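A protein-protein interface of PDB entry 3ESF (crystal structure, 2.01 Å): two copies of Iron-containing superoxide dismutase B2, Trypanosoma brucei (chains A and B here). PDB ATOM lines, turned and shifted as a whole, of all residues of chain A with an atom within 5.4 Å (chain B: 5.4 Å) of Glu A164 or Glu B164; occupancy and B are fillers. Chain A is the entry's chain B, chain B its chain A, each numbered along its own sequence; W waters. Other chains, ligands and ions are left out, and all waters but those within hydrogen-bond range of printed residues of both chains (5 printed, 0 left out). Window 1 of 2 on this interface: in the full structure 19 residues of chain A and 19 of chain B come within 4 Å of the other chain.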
ATOM      1  N   HIS A  32      10.260  -0.414  10.070  1.00  0.00           N
ATOM      2  CA  HIS A  32      10.893  -0.082   8.788  1.00  0.00           C
ATOM      3  C   HIS A  32      10.438   1.244   8.188  1.00  0.00           C
ATOM      4  O   HIS A  32      11.258   2.128   7.928  1.00  0.00           O
ATOM      5  CB  HIS A  32      10.735  -1.220   7.816  1.00  0.00           C
ATOM      6  CG  HIS A  32      11.443  -2.460   8.259  1.00  0.00           C
ATOM      7  ND1 HIS A  32      12.812  -2.610   8.161  1.00  0.00           N
ATOM      8  CD2 HIS A  32      10.972  -3.598   8.822  1.00  0.00           C
ATOM      9  CE1 HIS A  32      13.151  -3.789   8.656  1.00  0.00           C
ATOM     10  NE2 HIS A  32      12.055  -4.406   9.059  1.00  0.00           N
ATOM     11  N   SER A 123      16.441  -7.148  -2.679  1.00  0.00           N
ATOM     12  CA  SER A 123      15.423  -6.217  -2.189  1.00  0.00           C
ATOM     13  C   SER A 123      14.852  -5.381  -3.341  1.00  0.00           C
ATOM     14  O   SER A 123      15.601  -4.823  -4.119  1.00  0.00           O
ATOM     15  CB  SER A 123      16.040  -5.238  -1.163  1.00  0.00           C
ATOM     16  OG  SER A 123      16.469  -5.866   0.041  1.00  0.00           O
ATOM     17  N   VAL A 162       8.658  -6.279  -2.098  1.00  0.00           N
ATOM     18  CA  VAL A 162       9.247  -7.633  -2.057  1.00  0.00           C
ATOM     19  C   VAL A 162      10.617  -7.693  -1.326  1.00  0.00           C
ATOM     20  O   VAL A 162      11.329  -8.698  -1.381  1.00  0.00           O
ATOM     21  CB  VAL A 162       9.271  -8.384  -3.453  1.00  0.00           C
ATOM     22  CG1 VAL A 162       7.879  -8.557  -4.009  1.00  0.00           C
ATOM     23  CG2 VAL A 162      10.168  -7.678  -4.492  1.00  0.00           C
ATOM     24  N   TRP A 163      10.961  -6.620  -0.623  1.00  0.00           N
ATOM     25  CA  TRP A 163      11.930  -6.703   0.453  1.00  0.00           C
ATOM     26  C   TRP A 163      11.504  -7.836   1.399  1.00  0.00           C
ATOM     27  O   TRP A 163      10.325  -7.939   1.731  1.00  0.00           O
ATOM     28  CB  TRP A 163      11.994  -5.400   1.260  1.00  0.00           C
ATOM     29  CG  TRP A 163      12.731  -4.271   0.617  1.00  0.00           C
ATOM     30  CD1 TRP A 163      12.418  -3.656  -0.563  1.00  0.00           C
ATOM     31  CD2 TRP A 163      13.856  -3.540   1.157  1.00  0.00           C
ATOM     32  NE1 TRP A 163      13.290  -2.628  -0.816  1.00  0.00           N
ATOM     33  CE2 TRP A 163      14.180  -2.529   0.223  1.00  0.00           C
ATOM     34  CE3 TRP A 163      14.649  -3.676   2.316  1.00  0.00           C
ATOM     35  CZ2 TRP A 163      15.269  -1.658   0.401  1.00  0.00           C
ATOM     36  CZ3 TRP A 163      15.703  -2.791   2.508  1.00  0.00           C
ATOM     37  CH2 TRP A 163      16.002  -1.794   1.559  1.00  0.00           C
ATOM     38  N   GLU A 164      12.457  -8.652   1.843  1.00  0.00           N
ATOM     39  CA  GLU A 164      12.173  -9.749   2.781  1.00  0.00           C
ATOM     40  C   GLU A 164      11.398  -9.342   4.043  1.00  0.00           C
ATOM     41  O   GLU A 164      10.525 -10.085   4.480  1.00  0.00           O
ATOM     42  CB  GLU A 164      13.434 -10.521   3.135  1.00  0.00           C
ATOM     43  CG  GLU A 164      13.980 -11.194   1.894  1.00  0.00           C
ATOM     44  CD  GLU A 164      15.229 -11.980   2.101  1.00  0.00           C
ATOM     45  OE1 GLU A 164      16.189 -11.475   2.750  1.00  0.00           O
ATOM     46  OE2 GLU A 164      15.293 -13.102   1.533  1.00  0.00           O
ATOM     47  N   HIS A 165      11.698  -8.164   4.610  1.00  0.00           N
ATOM     48  CA  HIS A 165      10.920  -7.693   5.777  1.00  0.00           C
ATOM     49  C   HIS A 165       9.398  -7.521   5.565  1.00  0.00           C
ATOM     50  O   HIS A 165       8.643  -7.506   6.533  1.00  0.00           O
ATOM     51  CB  HIS A 165      11.514  -6.437   6.425  1.00  0.00           C
ATOM     52  CG  HIS A 165      11.327  -5.186   5.632  1.00  0.00           C
ATOM     53  ND1 HIS A 165      12.394  -4.465   5.132  1.00  0.00           N
ATOM     54  CD2 HIS A 165      10.215  -4.504   5.278  1.00  0.00           C
ATOM     55  CE1 HIS A 165      11.941  -3.402   4.491  1.00  0.00           C
ATOM     56  NE2 HIS A 165      10.620  -3.418   4.540  1.00  0.00           N
ATOM     57  N   ALA A 166       8.967  -7.351   4.318  1.00  0.00           N
ATOM     58  CA  ALA A 166       7.548  -7.207   3.999  1.00  0.00           C
ATOM     59  C   ALA A 166       6.727  -8.483   4.277  1.00  0.00           C
ATOM     60  O   ALA A 166       5.531  -8.403   4.573  1.00  0.00           O
ATOM     61  CB  ALA A 166       7.376  -6.754   2.545  1.00  0.00           C
ATOM     62  N   TYR A 167       7.375  -9.648   4.193  1.00  0.00           N
ATOM     63  CA  TYR A 167       6.681 -10.936   4.291  1.00  0.00           C
ATOM     64  C   TYR A 167       7.313 -11.952   5.225  1.00  0.00           C
ATOM     65  O   TYR A 167       6.711 -13.013   5.447  1.00  0.00           O
ATOM     66  CB  TYR A 167       6.528 -11.585   2.909  1.00  0.00           C
ATOM     67  CG  TYR A 167       7.810 -11.791   2.116  1.00  0.00           C
ATOM     68  CD1 TYR A 167       8.577 -12.972   2.278  1.00  0.00           C
ATOM     69  CD2 TYR A 167       8.275 -10.821   1.231  1.00  0.00           C
ATOM     70  CE1 TYR A 167       9.735 -13.194   1.564  1.00  0.00           C
ATOM     71  CE2 TYR A 167       9.475 -11.035   0.487  1.00  0.00           C
ATOM     72  CZ  TYR A 167      10.180 -12.224   0.652  1.00  0.00           C
ATOM     73  OH  TYR A 167      11.347 -12.477  -0.037  1.00  0.00           O
ATOM     74  N   TYR A 168       8.494 -11.653   5.774  1.00  0.00           N
ATOM     75  CA  TYR A 168       9.252 -12.691   6.487  1.00  0.00           C
ATOM     76  C   TYR A 168       8.563 -13.209   7.761  1.00  0.00           C
ATOM     77  O   TYR A 168       8.650 -14.396   8.055  1.00  0.00           O
ATOM     78  CB  TYR A 168      10.742 -12.309   6.746  1.00  0.00           C
ATOM     79  CG  TYR A 168      11.628 -13.528   6.534  1.00  0.00           C
ATOM     80  CD1 TYR A 168      12.043 -13.880   5.251  1.00  0.00           C
ATOM     81  CD2 TYR A 168      11.979 -14.368   7.592  1.00  0.00           C
ATOM     82  CE1 TYR A 168      12.799 -15.006   5.015  1.00  0.00           C
ATOM     83  CE2 TYR A 168      12.736 -15.518   7.360  1.00  0.00           C
ATOM     84  CZ  TYR A 168      13.136 -15.829   6.056  1.00  0.00           C
ATOM     85  OH  TYR A 168      13.885 -16.951   5.807  1.00  0.00           O
ATOM     86  N   ILE A 169       7.879 -12.328   8.493  1.00  0.00           N
ATOM     87  CA  ILE A 169       7.161 -12.732   9.713  1.00  0.00           C
ATOM     88  C   ILE A 169       6.048 -13.755   9.396  1.00  0.00           C
ATOM     89  O   ILE A 169       5.952 -14.808  10.017  1.00  0.00           O
ATOM     90  CB  ILE A 169       6.608 -11.489  10.516  1.00  0.00           C
ATOM     91  CG1 ILE A 169       7.761 -10.745  11.219  1.00  0.00           C
ATOM     92  CG2 ILE A 169       5.527 -11.907  11.531  1.00  0.00           C
ATOM     93  CD1 ILE A 169       7.459  -9.276  11.582  1.00  0.00           C
ATOM     94  N   ARG A 175       7.972 -16.314  -0.586  1.00  0.00           N
ATOM     95  CA  ARG A 175       7.510 -15.127  -1.304  1.00  0.00           C
ATOM     96  C   ARG A 175       6.358 -15.442  -2.278  1.00  0.00           C
ATOM     97  O   ARG A 175       5.438 -14.627  -2.405  1.00  0.00           O
ATOM     98  CB  ARG A 175       8.658 -14.422  -2.046  1.00  0.00           C
ATOM     99  CG  ARG A 175       8.236 -13.007  -2.530  1.00  0.00           C
ATOM    100  CD  ARG A 175       9.190 -12.290  -3.448  1.00  0.00           C
ATOM    101  NE  ARG A 175      10.588 -12.184  -2.979  1.00  0.00           N
ATOM    102  CZ  ARG A 175      11.573 -11.709  -3.744  1.00  0.00           C
ATOM    103  NH1 ARG A 175      11.308 -11.284  -4.960  1.00  0.00           N
ATOM    104  NH2 ARG A 175      12.815 -11.652  -3.300  1.00  0.00           N
ATOM    105  N   HIS B  32      16.880 -21.031   2.104  1.00  0.00           N
ATOM    106  CA  HIS B  32      17.650 -20.120   1.258  1.00  0.00           C
ATOM    107  C   HIS B  32      18.883 -20.739   0.635  1.00  0.00           C
ATOM    108  O   HIS B  32      18.992 -20.748  -0.592  1.00  0.00           O
ATOM    109  CB  HIS B  32      17.984 -18.790   1.966  1.00  0.00           C
ATOM    110  CG  HIS B  32      16.761 -18.049   2.405  1.00  0.00           C
ATOM    111  ND1 HIS B  32      16.021 -17.274   1.539  1.00  0.00           N
ATOM    112  CD2 HIS B  32      16.091 -18.048   3.583  1.00  0.00           C
ATOM    113  CE1 HIS B  32      14.975 -16.782   2.180  1.00  0.00           C
ATOM    114  NE2 HIS B  32      14.985 -17.246   3.418  1.00  0.00           N
ATOM    115  N   SER B 123      19.917  -5.765   0.278  1.00  0.00           N
ATOM    116  CA  SER B 123      20.485  -7.091   0.490  1.00  0.00           C
ATOM    117  C   SER B 123      21.974  -7.075   0.163  1.00  0.00           C
ATOM    118  O   SER B 123      22.370  -6.546  -0.906  1.00  0.00           O
ATOM    119  CB  SER B 123      19.766  -8.158  -0.385  1.00  0.00           C
ATOM    120  OG  SER B 123      18.347  -8.149  -0.189  1.00  0.00           O
ATOM    121  N   VAL B 162      24.060 -10.002   5.533  1.00  0.00           N
ATOM    122  CA  VAL B 162      23.103  -8.977   6.043  1.00  0.00           C
ATOM    123  C   VAL B 162      21.826  -8.849   5.192  1.00  0.00           C
ATOM    124  O   VAL B 162      21.072  -7.878   5.320  1.00  0.00           O
ATOM    125  CB  VAL B 162      23.762  -7.601   6.310  1.00  0.00           C
ATOM    126  CG1 VAL B 162      24.876  -7.735   7.314  1.00  0.00           C
ATOM    127  CG2 VAL B 162      24.254  -6.924   4.987  1.00  0.00           C
ATOM    128  N   TRP B 163      21.576  -9.820   4.306  1.00  0.00           N
ATOM    129  CA  TRP B 163      20.219 -10.017   3.790  1.00  0.00           C
ATOM    130  C   TRP B 163      19.302 -10.191   5.007  1.00  0.00           C
ATOM    131  O   TRP B 163      19.687 -10.858   5.983  1.00  0.00           O
ATOM    132  CB  TRP B 163      20.125 -11.311   2.966  1.00  0.00           C
ATOM    133  CG  TRP B 163      20.722 -11.265   1.578  1.00  0.00           C
ATOM    134  CD1 TRP B 163      22.026 -10.954   1.227  1.00  0.00           C
ATOM    135  CD2 TRP B 163      20.045 -11.596   0.358  1.00  0.00           C
ATOM    136  NE1 TRP B 163      22.169 -11.053  -0.149  1.00  0.00           N
ATOM    137  CE2 TRP B 163      20.973 -11.440  -0.701  1.00  0.00           C
ATOM    138  CE3 TRP B 163      18.740 -12.011   0.059  1.00  0.00           C
ATOM    139  CZ2 TRP B 163      20.631 -11.688  -2.055  1.00  0.00           C
ATOM    140  CZ3 TRP B 163      18.395 -12.245  -1.271  1.00  0.00           C
ATOM    141  CH2 TRP B 163      19.350 -12.103  -2.314  1.00  0.00           C
ATOM    142  N   GLU B 164      18.089  -9.656   4.914  1.00  0.00           N
ATOM    143  CA  GLU B 164      17.147  -9.676   5.996  1.00  0.00           C
ATOM    144  C   GLU B 164      16.819 -11.084   6.491  1.00  0.00           C
ATOM    145  O   GLU B 164      16.578 -11.253   7.677  1.00  0.00           O
ATOM    146  CB  GLU B 164      15.882  -8.882   5.670  1.00  0.00           C
ATOM    147  CG  GLU B 164      16.153  -7.396   5.758  1.00  0.00           C
ATOM    148  CD  GLU B 164      15.045  -6.501   5.231  1.00  0.00           C
ATOM    149  OE1 GLU B 164      14.290  -6.892   4.339  1.00  0.00           O
ATOM    150  OE2 GLU B 164      14.921  -5.368   5.716  1.00  0.00           O
ATOM    151  N   HIS B 165      16.803 -12.075   5.578  1.00  0.00           N
ATOM    152  CA  HIS B 165      16.525 -13.463   5.973  1.00  0.00           C
ATOM    153  C   HIS B 165      17.571 -14.085   6.906  1.00  0.00           C
ATOM    154  O   HIS B 165      17.273 -15.075   7.583  1.00  0.00           O
ATOM    155  CB  HIS B 165      16.285 -14.373   4.755  1.00  0.00           C
ATOM    156  CG  HIS B 165      17.507 -14.652   3.940  1.00  0.00           C
ATOM    157  ND1 HIS B 165      17.576 -14.377   2.592  1.00  0.00           N
ATOM    158  CD2 HIS B 165      18.705 -15.181   4.275  1.00  0.00           C
ATOM    159  CE1 HIS B 165      18.753 -14.755   2.125  1.00  0.00           C
ATOM    160  NE2 HIS B 165      19.467 -15.220   3.137  1.00  0.00           N
ATOM    161  N   ALA B 166      18.782 -13.515   6.933  1.00  0.00           N
ATOM    162  CA  ALA B 166      19.829 -13.969   7.831  1.00  0.00           C
ATOM    163  C   ALA B 166      19.462 -13.739   9.301  1.00  0.00           C
ATOM    164  O   ALA B 166      19.907 -14.493  10.181  1.00  0.00           O
ATOM    165  CB  ALA B 166      21.147 -13.314   7.512  1.00  0.00           C
ATOM    166  N   TYR B 167      18.648 -12.720   9.567  1.00  0.00           N
ATOM    167  CA  TYR B 167      18.448 -12.298  10.958  1.00  0.00           C
ATOM    168  C   TYR B 167      17.000 -12.044  11.334  1.00  0.00           C
ATOM    169  O   TYR B 167      16.707 -11.840  12.521  1.00  0.00           O
ATOM    170  CB  TYR B 167      19.325 -11.079  11.278  1.00  0.00           C
ATOM    171  CG  TYR B 167      19.092  -9.856  10.391  1.00  0.00           C
ATOM    172  CD1 TYR B 167      18.052  -8.957  10.687  1.00  0.00           C
ATOM    173  CD2 TYR B 167      19.892  -9.598   9.271  1.00  0.00           C
ATOM    174  CE1 TYR B 167      17.799  -7.834   9.892  1.00  0.00           C
ATOM    175  CE2 TYR B 167      19.662  -8.439   8.458  1.00  0.00           C
ATOM    176  CZ  TYR B 167      18.588  -7.579   8.804  1.00  0.00           C
ATOM    177  OH  TYR B 167      18.300  -6.443   8.102  1.00  0.00           O
ATOM    178  N   TYR B 168      16.092 -12.094  10.348  1.00  0.00           N
ATOM    179  CA  TYR B 168      14.708 -11.647  10.596  1.00  0.00           C
ATOM    180  C   TYR B 168      13.937 -12.469  11.641  1.00  0.00           C
ATOM    181  O   TYR B 168      13.155 -11.910  12.420  1.00  0.00           O
ATOM    182  CB  TYR B 168      13.877 -11.454   9.310  1.00  0.00           C
ATOM    183  CG  TYR B 168      13.073 -10.176   9.427  1.00  0.00           C
ATOM    184  CD1 TYR B 168      13.662  -8.927   9.133  1.00  0.00           C
ATOM    185  CD2 TYR B 168      11.761 -10.198   9.913  1.00  0.00           C
ATOM    186  CE1 TYR B 168      12.952  -7.733   9.285  1.00  0.00           C
ATOM    187  CE2 TYR B 168      11.042  -9.013  10.084  1.00  0.00           C
ATOM    188  CZ  TYR B 168      11.647  -7.788   9.767  1.00  0.00           C
ATOM    189  OH  TYR B 168      10.949  -6.628   9.972  1.00  0.00           O
ATOM    190  N   ILE B 169      14.182 -13.776  11.672  1.00  0.00           N
ATOM    191  CA  ILE B 169      13.508 -14.680  12.626  1.00  0.00           C
ATOM    192  C   ILE B 169      13.914 -14.352  14.071  1.00  0.00           C
ATOM    193  O   ILE B 169      13.045 -14.261  14.939  1.00  0.00           O
ATOM    194  CB  ILE B 169      13.731 -16.192  12.277  1.00  0.00           C
ATOM    195  CG1 ILE B 169      12.994 -16.541  10.968  1.00  0.00           C
ATOM    196  CG2 ILE B 169      13.282 -17.108  13.411  1.00  0.00           C
ATOM    197  CD1 ILE B 169      13.301 -17.918  10.388  1.00  0.00           C
HETATM  198  O   HOH W   1       8.407  -6.063   8.916  1.00  0.00           O
HETATM  199  O   HOH W   2      15.213  -7.462   1.787  1.00  0.00           O
HETATM  200  O   HOH W   3      17.189  -9.153   2.076  1.00  0.00           O
HETATM  201  O   HOH W   4      19.098  -5.756  -2.466  1.00  0.00           O
HETATM  202  O   HOH W   5      16.195 -17.671   7.081  1.00  0.00           O
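Water W3 lies within hydrogen-bond range of OE1 of Glu A164 (2.6 Å), OG of Ser B123 (2.7 Å) and N of Glu B164 (3.0 Å). Water W2 lies within hydrogen-bond range of OG of Ser A123, OE1 of Glu B164 and N of Glu A164. Water W5 lies within hydrogen-bond range of OH of Tyr A168 (2.7 Å) and O of His B165 (2.9 Å). Water W1 lies within hydrogen-bond range of the backbone carbonyl oxygen (O) of His A165 (2.8 Å) and the side-chain hydroxyl (OH) of Tyr B168 (2.8 Å). Water W4 lies within hydrogen-bond range of N of Ser B123 and N of Ser A123.
Hydrophobic or aromatic side chains of chain A that line the printed part of chain B: His A32, Trp A163, His A165, Tyr A168 and Ile A169. Among the printed residues, 15 pairs touch across the chains. Among the printed residues, no Asp or Glu carboxylate lies within 4 Å of a Lys or Arg side-chain nitrogen of the other chain.
His A32 touches Glu B164, and with the chains exchanged Glu A164 touches His B32. Ser B123 touches its own counterpart, Ser A123. Glu A164 touches His B165, and with the chains exchanged His A165 touches Glu B164. Tyr B168 touches its own counterpart, Tyr A168. 10 positions are printed for both chains. Of the 15 pairs that touch across the chains among the printed residues, 15 have their exchanged pair printed and touching as well.
Printed residues of chain B within 4 Å of Ser A123: Ser B123 (3.0 Å). Of the printed residues of chain B, Ile A169 touches Tyr B168. Of chain A, only His A32, Trp A163, Glu A164 and His A165 come within 4 Å of Glu B164. The nearest printed residue of chain A that does not touch His B165 is His A165 (6.5 Å).
ND1 of His B32 sits at hydrogen-bond distance from ND1 of His B165.
Glu B164 touches His A32 (OE2 to CE1, 3.8 Å). Trp A163 touches Glu B164. OE2 of Glu A164 touches CE1 of His B32, 3.7 Å away. OE1 of Glu A164 touches CE3 of Trp B163 (3.7 Å). His A165 touches Tyr B168. Tyr A168 touches His B165. Tyr A168 touches Tyr B168 (CD2 to CB, 3.9 Å). Tyr A168 touches Ile B169. Ile A169 touches Tyr B168.
A ring nitrogen (NE2) of His B32 lies within hydrogen-bond range of the side-chain hydroxyl (OH) of Tyr A168 (2.6 Å). OG of Ser A123 is in hydrogen-bond range of OG of Ser B123 (3.0 Å). N of Glu B164 lies within hydrogen-bond range of OE1 of Glu A164 (3.4 Å). OE2 of Glu B164 is in hydrogen-bond range of ND1 of His A165, 2.7 Å away. ND1 of His B165 lies within hydrogen-bond range of OE2 of Glu A164. A ring nitrogen (NE2) of His A32 is in hydrogen-bond range of the side-chain hydroxyl of Tyr B168 (2.6 Å).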
